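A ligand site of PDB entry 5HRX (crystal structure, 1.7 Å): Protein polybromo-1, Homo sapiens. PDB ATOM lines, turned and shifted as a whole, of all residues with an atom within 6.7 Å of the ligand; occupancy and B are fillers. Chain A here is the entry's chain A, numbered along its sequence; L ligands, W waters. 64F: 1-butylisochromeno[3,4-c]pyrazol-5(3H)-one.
ND2 of Asn 97 lies close to NAN of the ligand, at 3.0 Å.
An oxygen (OAK) of the ligand sits at hydrogen-bond distance from the backbone NH of Ala 93.
The backbone NH (N) of Met 62 is in hydrogen-bond range of the side-chain hydroxyl (OH) of Tyr 54.
The side-chain sulfur (SD) of Met 89 lies close to the backbone NH (N) of Met 64.
ND2 of Asn 97 is in hydrogen-bond range of O of Ala 93, at 2.9 Å.
The backbone NH (N) of Met 64 is in hydrogen-bond range of the backbone carbonyl oxygen (O) of Phe 42 (3.0 Å).
NH1 of Arg 44 is in salt-bridge range of OD2 of Asp 63, at 2.8 Å.
The side-chain carboxylate (OD2) of Asp 63 lies within hydrogen-bond range of the backbone NH (N) of Leu 45, 2.9 Å away.
Water W1 bridges the side-chain amide oxygen (OD1) of Asn 97 (2.7 Å) and a nitrogen (NAM) of the ligand (2.8 Å).
Water W2 lies within hydrogen-bond range of OH of Tyr 54 (2.6 Å), O of Met 62 (2.7 Å), OAK of the ligand (2.9 Å) and ND2 of Asn 92 (3.1 Å).
The backbone carbonyl oxygen (O) of Met 89 sits close to an oxygen (OAK) of the ligand, 3.4 Å away.
Ile 41 touches the ligand (O to CAB, 3.2 Å).
Phe 42 touches the ligand.
Arg 44 touches the ligand.
Leu 45 touches the ligand.
Leu 51 touches the ligand.
Tyr 54 touches the ligand (CE2 to CAJ, 3.7 Å).
Met 62 touches the ligand.
Asp 63 touches the ligand (CB to CAA, 3.6 Å).
Tyr 96 touches the ligand (CD2 to NAN, 3.6 Å).
Hydrophobic or aromatic side chains within 4 Å of the ligand: Phe 42, Leu 45, Leu 51, Tyr 54, Ala 93 and Tyr 96.
Of the 23 residues printed, 12 come within 4 Å of the ligand.
The nearest printed residue that does not touch the ligand is Asn 92 (4.1 Å).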
ATOM      1  N   ILE A  41     -25.078 -24.749   5.869  1.00  0.00           N
ATOM      2  CA  ILE A  41     -25.897 -23.793   4.994  1.00  0.00           C
ATOM      3  C   ILE A  41     -26.164 -24.391   3.618  1.00  0.00           C
ATOM      4  O   ILE A  41     -27.099 -23.910   2.919  1.00  0.00           O
ATOM      5  CB  ILE A  41     -25.291 -22.419   4.888  1.00  0.00           C
ATOM      6  CG1 ILE A  41     -24.011 -22.445   4.094  1.00  0.00           C
ATOM      7  CG2 ILE A  41     -25.101 -21.857   6.307  1.00  0.00           C
ATOM      8  CD1 ILE A  41     -24.203 -21.996   2.669  1.00  0.00           C
ATOM      9  N   PHE A  42     -25.418 -25.426   3.220  1.00  0.00           N
ATOM     10  CA  PHE A  42     -25.559 -26.032   1.904  1.00  0.00           C
ATOM     11  C   PHE A  42     -26.627 -27.120   1.793  1.00  0.00           C
ATOM     12  O   PHE A  42     -26.883 -27.614   0.683  1.00  0.00           O
ATOM     13  CB  PHE A  42     -24.177 -26.659   1.509  1.00  0.00           C
ATOM     14  CG  PHE A  42     -23.108 -25.612   1.257  1.00  0.00           C
ATOM     15  CD1 PHE A  42     -23.052 -24.904   0.051  1.00  0.00           C
ATOM     16  CD2 PHE A  42     -22.206 -25.259   2.243  1.00  0.00           C
ATOM     17  CE1 PHE A  42     -22.116 -23.903  -0.153  1.00  0.00           C
ATOM     18  CE2 PHE A  42     -21.234 -24.294   2.021  1.00  0.00           C
ATOM     19  CZ  PHE A  42     -21.175 -23.614   0.834  1.00  0.00           C
ATOM     20  N   LEU A  43     -27.222 -27.559   2.896  1.00  0.00           N
ATOM     21  CA  LEU A  43     -28.193 -28.626   2.874  1.00  0.00           C
ATOM     22  C   LEU A  43     -29.399 -28.331   1.997  1.00  0.00           C
ATOM     23  O   LEU A  43     -29.813 -29.144   1.174  1.00  0.00           O
ATOM     24  CB  LEU A  43     -28.606 -29.012   4.274  1.00  0.00           C
ATOM     25  CG  LEU A  43     -27.432 -29.450   5.214  1.00  0.00           C
ATOM     26  CD1 LEU A  43     -27.983 -29.858   6.582  1.00  0.00           C
ATOM     27  CD2 LEU A  43     -26.456 -30.486   4.643  1.00  0.00           C
ATOM     28  N   ARG A  44     -29.970 -27.154   2.172  1.00  0.00           N
ATOM     29  CA  ARG A  44     -31.172 -26.754   1.480  1.00  0.00           C
ATOM     30  C   ARG A  44     -31.152 -25.243   1.071  1.00  0.00           C
ATOM     31  O   ARG A  44     -31.022 -24.363   1.884  1.00  0.00           O
ATOM     32  CB  ARG A  44     -32.405 -27.037   2.337  1.00  0.00           C
ATOM     33  CG  ARG A  44     -33.711 -26.875   1.547  1.00  0.00           C
ATOM     34  CD  ARG A  44     -33.917 -28.074   0.637  1.00  0.00           C
ATOM     35  NE  ARG A  44     -35.189 -27.909  -0.049  1.00  0.00           N
ATOM     36  CZ  ARG A  44     -35.391 -27.458  -1.274  1.00  0.00           C
ATOM     37  NH1 ARG A  44     -34.397 -27.130  -2.118  1.00  0.00           N
ATOM     38  NH2 ARG A  44     -36.675 -27.358  -1.682  1.00  0.00           N
ATOM     39  N   LEU A  45     -31.218 -25.019  -0.222  1.00  0.00           N
ATOM     40  CA  LEU A  45     -31.390 -23.667  -0.771  1.00  0.00           C
ATOM     41  C   LEU A  45     -32.668 -23.004  -0.237  1.00  0.00           C
ATOM     42  O   LEU A  45     -33.697 -23.681  -0.170  1.00  0.00           O
ATOM     43  CB  LEU A  45     -31.528 -23.716  -2.289  1.00  0.00           C
ATOM     44  CG  LEU A  45     -30.247 -23.620  -3.079  1.00  0.00           C
ATOM     45  CD1 LEU A  45     -30.504 -24.071  -4.519  1.00  0.00           C
ATOM     46  CD2 LEU A  45     -29.589 -22.198  -3.029  1.00  0.00           C
ATOM     47  N   PRO A  46     -32.562 -21.710   0.137  1.00  0.00           N
ATOM     48  CA  PRO A  46     -33.773 -20.908   0.370  1.00  0.00           C
ATOM     49  C   PRO A  46     -34.635 -20.762  -0.877  1.00  0.00           C
ATOM     50  O   PRO A  46     -34.228 -21.172  -1.993  1.00  0.00           O
ATOM     51  CB  PRO A  46     -33.215 -19.561   0.811  1.00  0.00           C
ATOM     52  CG  PRO A  46     -31.796 -19.877   1.333  1.00  0.00           C
ATOM     53  CD  PRO A  46     -31.356 -20.857   0.270  1.00  0.00           C
ATOM     54  N   GLU A  50     -36.734 -15.771  -0.962  1.00  0.00           N
ATOM     55  CA  GLU A  50     -35.730 -15.645   0.114  1.00  0.00           C
ATOM     56  C   GLU A  50     -34.319 -15.290  -0.345  1.00  0.00           C
ATOM     57  O   GLU A  50     -33.598 -14.588   0.377  1.00  0.00           O
ATOM     58  CB  GLU A  50     -35.745 -16.928   0.953  1.00  0.00           C
ATOM     59  CG  GLU A  50     -36.990 -17.141   1.811  1.00  0.00           C
ATOM     60  CD  GLU A  50     -36.990 -18.497   2.528  1.00  0.00           C
ATOM     61  OE1 GLU A  50     -36.521 -19.468   1.960  1.00  0.00           O
ATOM     62  OE2 GLU A  50     -37.481 -18.561   3.702  1.00  0.00           O
ATOM     63  N   LEU A  51     -33.924 -15.773  -1.525  1.00  0.00           N
ATOM     64  CA  LEU A  51     -32.570 -15.570  -2.034  1.00  0.00           C
ATOM     65  C   LEU A  51     -32.668 -15.320  -3.499  1.00  0.00           C
ATOM     66  O   LEU A  51     -32.170 -16.043  -4.317  1.00  0.00           O
ATOM     67  CB  LEU A  51     -31.704 -16.815  -1.738  1.00  0.00           C
ATOM     68  CG  LEU A  51     -30.183 -16.601  -1.772  1.00  0.00           C
ATOM     69  CD1 LEU A  51     -29.683 -15.810  -0.562  1.00  0.00           C
ATOM     70  CD2 LEU A  51     -29.531 -17.967  -1.847  1.00  0.00           C
ATOM     71  N   TYR A  54     -29.495 -15.200  -5.976  1.00  0.00           N
ATOM     72  CA  TYR A  54     -28.890 -16.517  -6.365  1.00  0.00           C
ATOM     73  C   TYR A  54     -29.573 -17.051  -7.621  1.00  0.00           C
ATOM     74  O   TYR A  54     -28.912 -17.386  -8.574  1.00  0.00           O
ATOM     75  CB  TYR A  54     -29.056 -17.558  -5.229  1.00  0.00           C
ATOM     76  CG  TYR A  54     -28.694 -18.953  -5.579  1.00  0.00           C
ATOM     77  CD1 TYR A  54     -29.589 -19.802  -6.160  1.00  0.00           C
ATOM     78  CD2 TYR A  54     -27.394 -19.471  -5.294  1.00  0.00           C
ATOM     79  CE1 TYR A  54     -29.247 -21.137  -6.469  1.00  0.00           C
ATOM     80  CE2 TYR A  54     -27.072 -20.781  -5.584  1.00  0.00           C
ATOM     81  CZ  TYR A  54     -28.007 -21.600  -6.187  1.00  0.00           C
ATOM     82  OH  TYR A  54     -27.700 -22.919  -6.529  1.00  0.00           O
ATOM     83  N   ILE A  58     -27.640 -17.986 -11.134  1.00  0.00           N
ATOM     84  CA  ILE A  58     -27.214 -19.396 -11.259  1.00  0.00           C
ATOM     85  C   ILE A  58     -28.231 -20.130 -12.166  1.00  0.00           C
ATOM     86  O   ILE A  58     -29.426 -20.194 -11.861  1.00  0.00           O
ATOM     87  CB  ILE A  58     -27.192 -20.032  -9.833  1.00  0.00           C
ATOM     88  CG1 ILE A  58     -26.163 -19.317  -8.946  1.00  0.00           C
ATOM     89  CG2 ILE A  58     -27.007 -21.513  -9.869  1.00  0.00           C
ATOM     90  CD1 ILE A  58     -24.731 -19.352  -9.477  1.00  0.00           C
ATOM     91  N   MET A  62     -28.434 -26.056  -7.154  1.00  0.00           N
ATOM     92  CA  MET A  62     -28.058 -27.310  -6.565  1.00  0.00           C
ATOM     93  C   MET A  62     -27.883 -27.155  -5.021  1.00  0.00           C
ATOM     94  O   MET A  62     -27.348 -26.164  -4.544  1.00  0.00           O
ATOM     95  CB  MET A  62     -26.744 -27.742  -7.220  1.00  0.00           C
ATOM     96  CG  MET A  62     -26.301 -29.160  -6.852  1.00  0.00           C
ATOM     97  SD  MET A  62     -27.464 -30.503  -7.209  1.00  0.00           S
ATOM     98  CE  MET A  62     -27.319 -30.435  -8.992  1.00  0.00           C
ATOM     99  N   ASP A  63     -28.354 -28.118  -4.267  1.00  0.00           N
ATOM    100  CA  ASP A  63     -28.128 -28.225  -2.808  1.00  0.00           C
ATOM    101  C   ASP A  63     -27.906 -29.673  -2.398  1.00  0.00           C
ATOM    102  O   ASP A  63     -28.051 -30.577  -3.253  1.00  0.00           O
ATOM    103  CB  ASP A  63     -29.298 -27.462  -2.041  1.00  0.00           C
ATOM    104  CG  ASP A  63     -30.680 -28.116  -2.181  1.00  0.00           C
ATOM    105  OD1 ASP A  63     -30.844 -29.319  -2.556  1.00  0.00           O
ATOM    106  OD2 ASP A  63     -31.652 -27.303  -1.909  1.00  0.00           O
ATOM    107  N   MET A  64     -27.447 -29.901  -1.166  1.00  0.00           N
ATOM    108  CA  MET A  64     -27.113 -31.260  -0.724  1.00  0.00           C
ATOM    109  C   MET A  64     -28.359 -32.132  -0.610  1.00  0.00           C
ATOM    110  O   MET A  64     -28.255 -33.329  -0.833  1.00  0.00           O
ATOM    111  CB  MET A  64     -26.334 -31.212   0.523  1.00  0.00           C
ATOM    112  CG  MET A  64     -24.986 -30.585   0.269  1.00  0.00           C
ATOM    113  SD  MET A  64     -23.770 -30.659   1.616  1.00  0.00           S
ATOM    114  CE  MET A  64     -23.731 -32.381   1.992  1.00  0.00           C
ATOM    115  N   MET A  88     -20.598 -28.648  -9.057  1.00  0.00           N
ATOM    116  CA  MET A  88     -21.498 -27.641  -9.585  1.00  0.00           C
ATOM    117  C   MET A  88     -22.031 -26.801  -8.424  1.00  0.00           C
ATOM    118  O   MET A  88     -22.022 -25.572  -8.492  1.00  0.00           O
ATOM    119  CB  MET A  88     -22.660 -28.288 -10.310  1.00  0.00           C
ATOM    120  CG  MET A  88     -23.778 -27.297 -10.445  1.00  0.00           C
ATOM    121  SD  MET A  88     -23.594 -26.488 -12.009  1.00  0.00           S
ATOM    122  CE  MET A  88     -24.577 -27.854 -12.584  1.00  0.00           C
ATOM    123  N   MET A  89     -22.433 -27.472  -7.354  1.00  0.00           N
ATOM    124  CA  MET A  89     -22.825 -26.724  -6.145  1.00  0.00           C
ATOM    125  C   MET A  89     -21.783 -25.712  -5.658  1.00  0.00           C
ATOM    126  O   MET A  89     -22.091 -24.537  -5.351  1.00  0.00           O
ATOM    127  CB  MET A  89     -23.239 -27.699  -5.016  1.00  0.00           C
ATOM    128  CG  MET A  89     -23.889 -27.002  -3.809  1.00  0.00           C
ATOM    129  SD  MET A  89     -24.382 -28.130  -2.541  1.00  0.00           S
ATOM    130  CE  MET A  89     -22.759 -28.494  -1.874  1.00  0.00           C
ATOM    131  N   PHE A  90     -20.540 -26.130  -5.494  1.00  0.00           N
ATOM    132  CA  PHE A  90     -19.501 -25.241  -4.991  1.00  0.00           C
ATOM    133  C   PHE A  90     -19.131 -24.146  -5.999  1.00  0.00           C
ATOM    134  O   PHE A  90     -18.908 -23.013  -5.592  1.00  0.00           O
ATOM    135  CB  PHE A  90     -18.258 -26.051  -4.560  1.00  0.00           C
ATOM    136  CG  PHE A  90     -18.545 -27.076  -3.473  1.00  0.00           C
ATOM    137  CD1 PHE A  90     -19.223 -26.698  -2.319  1.00  0.00           C
ATOM    138  CD2 PHE A  90     -18.091 -28.410  -3.583  1.00  0.00           C
ATOM    139  CE1 PHE A  90     -19.470 -27.636  -1.286  1.00  0.00           C
ATOM    140  CE2 PHE A  90     -18.409 -29.331  -2.586  1.00  0.00           C
ATOM    141  CZ  PHE A  90     -19.080 -28.944  -1.451  1.00  0.00           C
ATOM    142  N   ASN A  91     -19.120 -24.469  -7.294  1.00  0.00           N
ATOM    143  CA  ASN A  91     -18.913 -23.472  -8.388  1.00  0.00           C
ATOM    144  C   ASN A  91     -20.031 -22.449  -8.330  1.00  0.00           C
ATOM    145  O   ASN A  91     -19.734 -21.285  -8.438  1.00  0.00           O
ATOM    146  CB  ASN A  91     -18.884 -24.120  -9.762  1.00  0.00           C
ATOM    147  CG  ASN A  91     -17.621 -24.834 -10.019  1.00  0.00           C
ATOM    148  OD1 ASN A  91     -16.586 -24.624  -9.318  1.00  0.00           O
ATOM    149  ND2 ASN A  91     -17.636 -25.720 -10.994  1.00  0.00           N
ATOM    150  N   ASN A  92     -21.277 -22.921  -8.143  1.00  0.00           N
ATOM    151  CA  ASN A  92     -22.435 -22.000  -8.012  1.00  0.00           C
ATOM    152  C   ASN A  92     -22.172 -21.062  -6.835  1.00  0.00           C
ATOM    153  O   ASN A  92     -22.263 -19.806  -6.960  1.00  0.00           O
ATOM    154  CB  ASN A  92     -23.769 -22.732  -7.800  1.00  0.00           C
ATOM    155  CG  ASN A  92     -24.293 -23.469  -9.010  1.00  0.00           C
ATOM    156  OD1 ASN A  92     -23.896 -23.227 -10.185  1.00  0.00           O
ATOM    157  ND2 ASN A  92     -25.247 -24.338  -8.763  1.00  0.00           N
ATOM    158  N   ALA A  93     -21.842 -21.598  -5.673  1.00  0.00           N
ATOM    159  CA  ALA A  93     -21.614 -20.738  -4.452  1.00  0.00           C
ATOM    160  C   ALA A  93     -20.547 -19.648  -4.753  1.00  0.00           C
ATOM    161  O   ALA A  93     -20.606 -18.542  -4.278  1.00  0.00           O
ATOM    162  CB  ALA A  93     -21.209 -21.648  -3.267  1.00  0.00           C
ATOM    163  N   CYS A  94     -19.420 -20.083  -5.402  1.00  0.00           N
ATOM    164  CA  CYS A  94     -18.331 -19.169  -5.707  1.00  0.00           C
ATOM    165  C   CYS A  94     -18.588 -18.261  -6.941  1.00  0.00           C
ATOM    166  O   CYS A  94     -17.779 -17.394  -7.250  1.00  0.00           O
ATOM    167  CB  CYS A  94     -17.074 -19.957  -5.926  1.00  0.00           C
ATOM    168  SG  CYS A  94     -16.545 -20.824  -4.419  1.00  0.00           S
ATOM    169  N   TYR A  96     -22.023 -16.968  -7.327  1.00  0.00           N
ATOM    170  CA  TYR A  96     -22.997 -16.026  -6.679  1.00  0.00           C
ATOM    171  C   TYR A  96     -22.349 -15.128  -5.634  1.00  0.00           C
ATOM    172  O   TYR A  96     -22.619 -13.955  -5.605  1.00  0.00           O
ATOM    173  CB  TYR A  96     -24.149 -16.815  -6.043  1.00  0.00           C
ATOM    174  CG  TYR A  96     -25.063 -15.931  -5.222  1.00  0.00           C
ATOM    175  CD1 TYR A  96     -25.619 -14.773  -5.778  1.00  0.00           C
ATOM    176  CD2 TYR A  96     -25.341 -16.221  -3.898  1.00  0.00           C
ATOM    177  CE1 TYR A  96     -26.411 -13.947  -5.019  1.00  0.00           C
ATOM    178  CE2 TYR A  96     -26.143 -15.390  -3.120  1.00  0.00           C
ATOM    179  CZ  TYR A  96     -26.668 -14.261  -3.725  1.00  0.00           C
ATOM    180  OH  TYR A  96     -27.385 -13.495  -2.882  1.00  0.00           O
ATOM    181  N   ASN A  97     -21.571 -15.691  -4.709  1.00  0.00           N
ATOM    182  CA  ASN A  97     -20.947 -14.962  -3.652  1.00  0.00           C
ATOM    183  C   ASN A  97     -19.603 -14.368  -4.048  1.00  0.00           C
ATOM    184  O   ASN A  97     -18.932 -14.845  -5.005  1.00  0.00           O
ATOM    185  CB  ASN A  97     -20.774 -15.868  -2.455  1.00  0.00           C
ATOM    186  CG  ASN A  97     -22.098 -16.354  -1.912  1.00  0.00           C
ATOM    187  OD1 ASN A  97     -22.772 -15.602  -1.117  1.00  0.00           O
ATOM    188  ND2 ASN A  97     -22.449 -17.605  -2.183  1.00  0.00           N
ATOM    189  N   ILE A 103     -19.256 -17.912   2.965  1.00  0.00           N
ATOM    190  CA  ILE A 103     -19.829 -19.042   2.269  1.00  0.00           C
ATOM    191  C   ILE A 103     -18.902 -19.435   1.094  1.00  0.00           C
ATOM    192  O   ILE A 103     -18.749 -20.657   0.763  1.00  0.00           O
ATOM    193  CB  ILE A 103     -21.224 -18.692   1.740  1.00  0.00           C
ATOM    194  CG1 ILE A 103     -22.125 -18.432   2.963  1.00  0.00           C
ATOM    195  CG2 ILE A 103     -21.801 -19.804   0.884  1.00  0.00           C
ATOM    196  CD1 ILE A 103     -23.153 -17.389   2.767  1.00  0.00           C
HETATM  197  CAG 64F L   1     -26.190 -20.560  -0.770  1.00  0.00           C
HETATM  198  CAD 64F L   1     -26.533 -21.892  -0.892  1.00  0.00           C
HETATM  199  CAC 64F L   1     -27.408 -22.603  -0.022  1.00  0.00           C
HETATM  200  CAB 64F L   1     -27.708 -23.963  -0.172  1.00  0.00           C
HETATM  201  CAA 64F L   1     -27.089 -24.705  -1.192  1.00  0.00           C
HETATM  202  CAF 64F L   1     -26.217 -24.031  -2.034  1.00  0.00           C
HETATM  203  CAE 64F L   1     -25.900 -22.668  -1.923  1.00  0.00           C
HETATM  204  CAJ 64F L   1     -25.039 -22.031  -2.817  1.00  0.00           C
HETATM  205  OAK 64F L   1     -24.440 -22.606  -3.753  1.00  0.00           O
HETATM  206  OAI 64F L   1     -24.745 -20.765  -2.661  1.00  0.00           O
HETATM  207  CAH 64F L   1     -25.292 -20.025  -1.645  1.00  0.00           C
HETATM  208  NAN 64F L   1     -25.135 -18.755  -1.409  1.00  0.00           N
HETATM  209  NAM 64F L   1     -25.843 -18.430  -0.390  1.00  0.00           N
HETATM  210  CAL 64F L   1     -26.500 -19.488   0.025  1.00  0.00           C
HETATM  211  CAO 64F L   1     -27.456 -19.394   1.198  1.00  0.00           C
HETATM  212  CAP 64F L   1     -27.325 -17.978   1.788  1.00  0.00           C
HETATM  213  CAQ 64F L   1     -28.380 -17.806   2.875  1.00  0.00           C
HETATM  214  CAR 64F L   1     -28.177 -16.437   3.560  1.00  0.00           C
HETATM  215  O   HOH W   1     -25.110 -15.788   0.279  1.00  0.00           O
HETATM  216  O   HOH W   2     -25.675 -24.324  -5.675  1.00  0.00           O
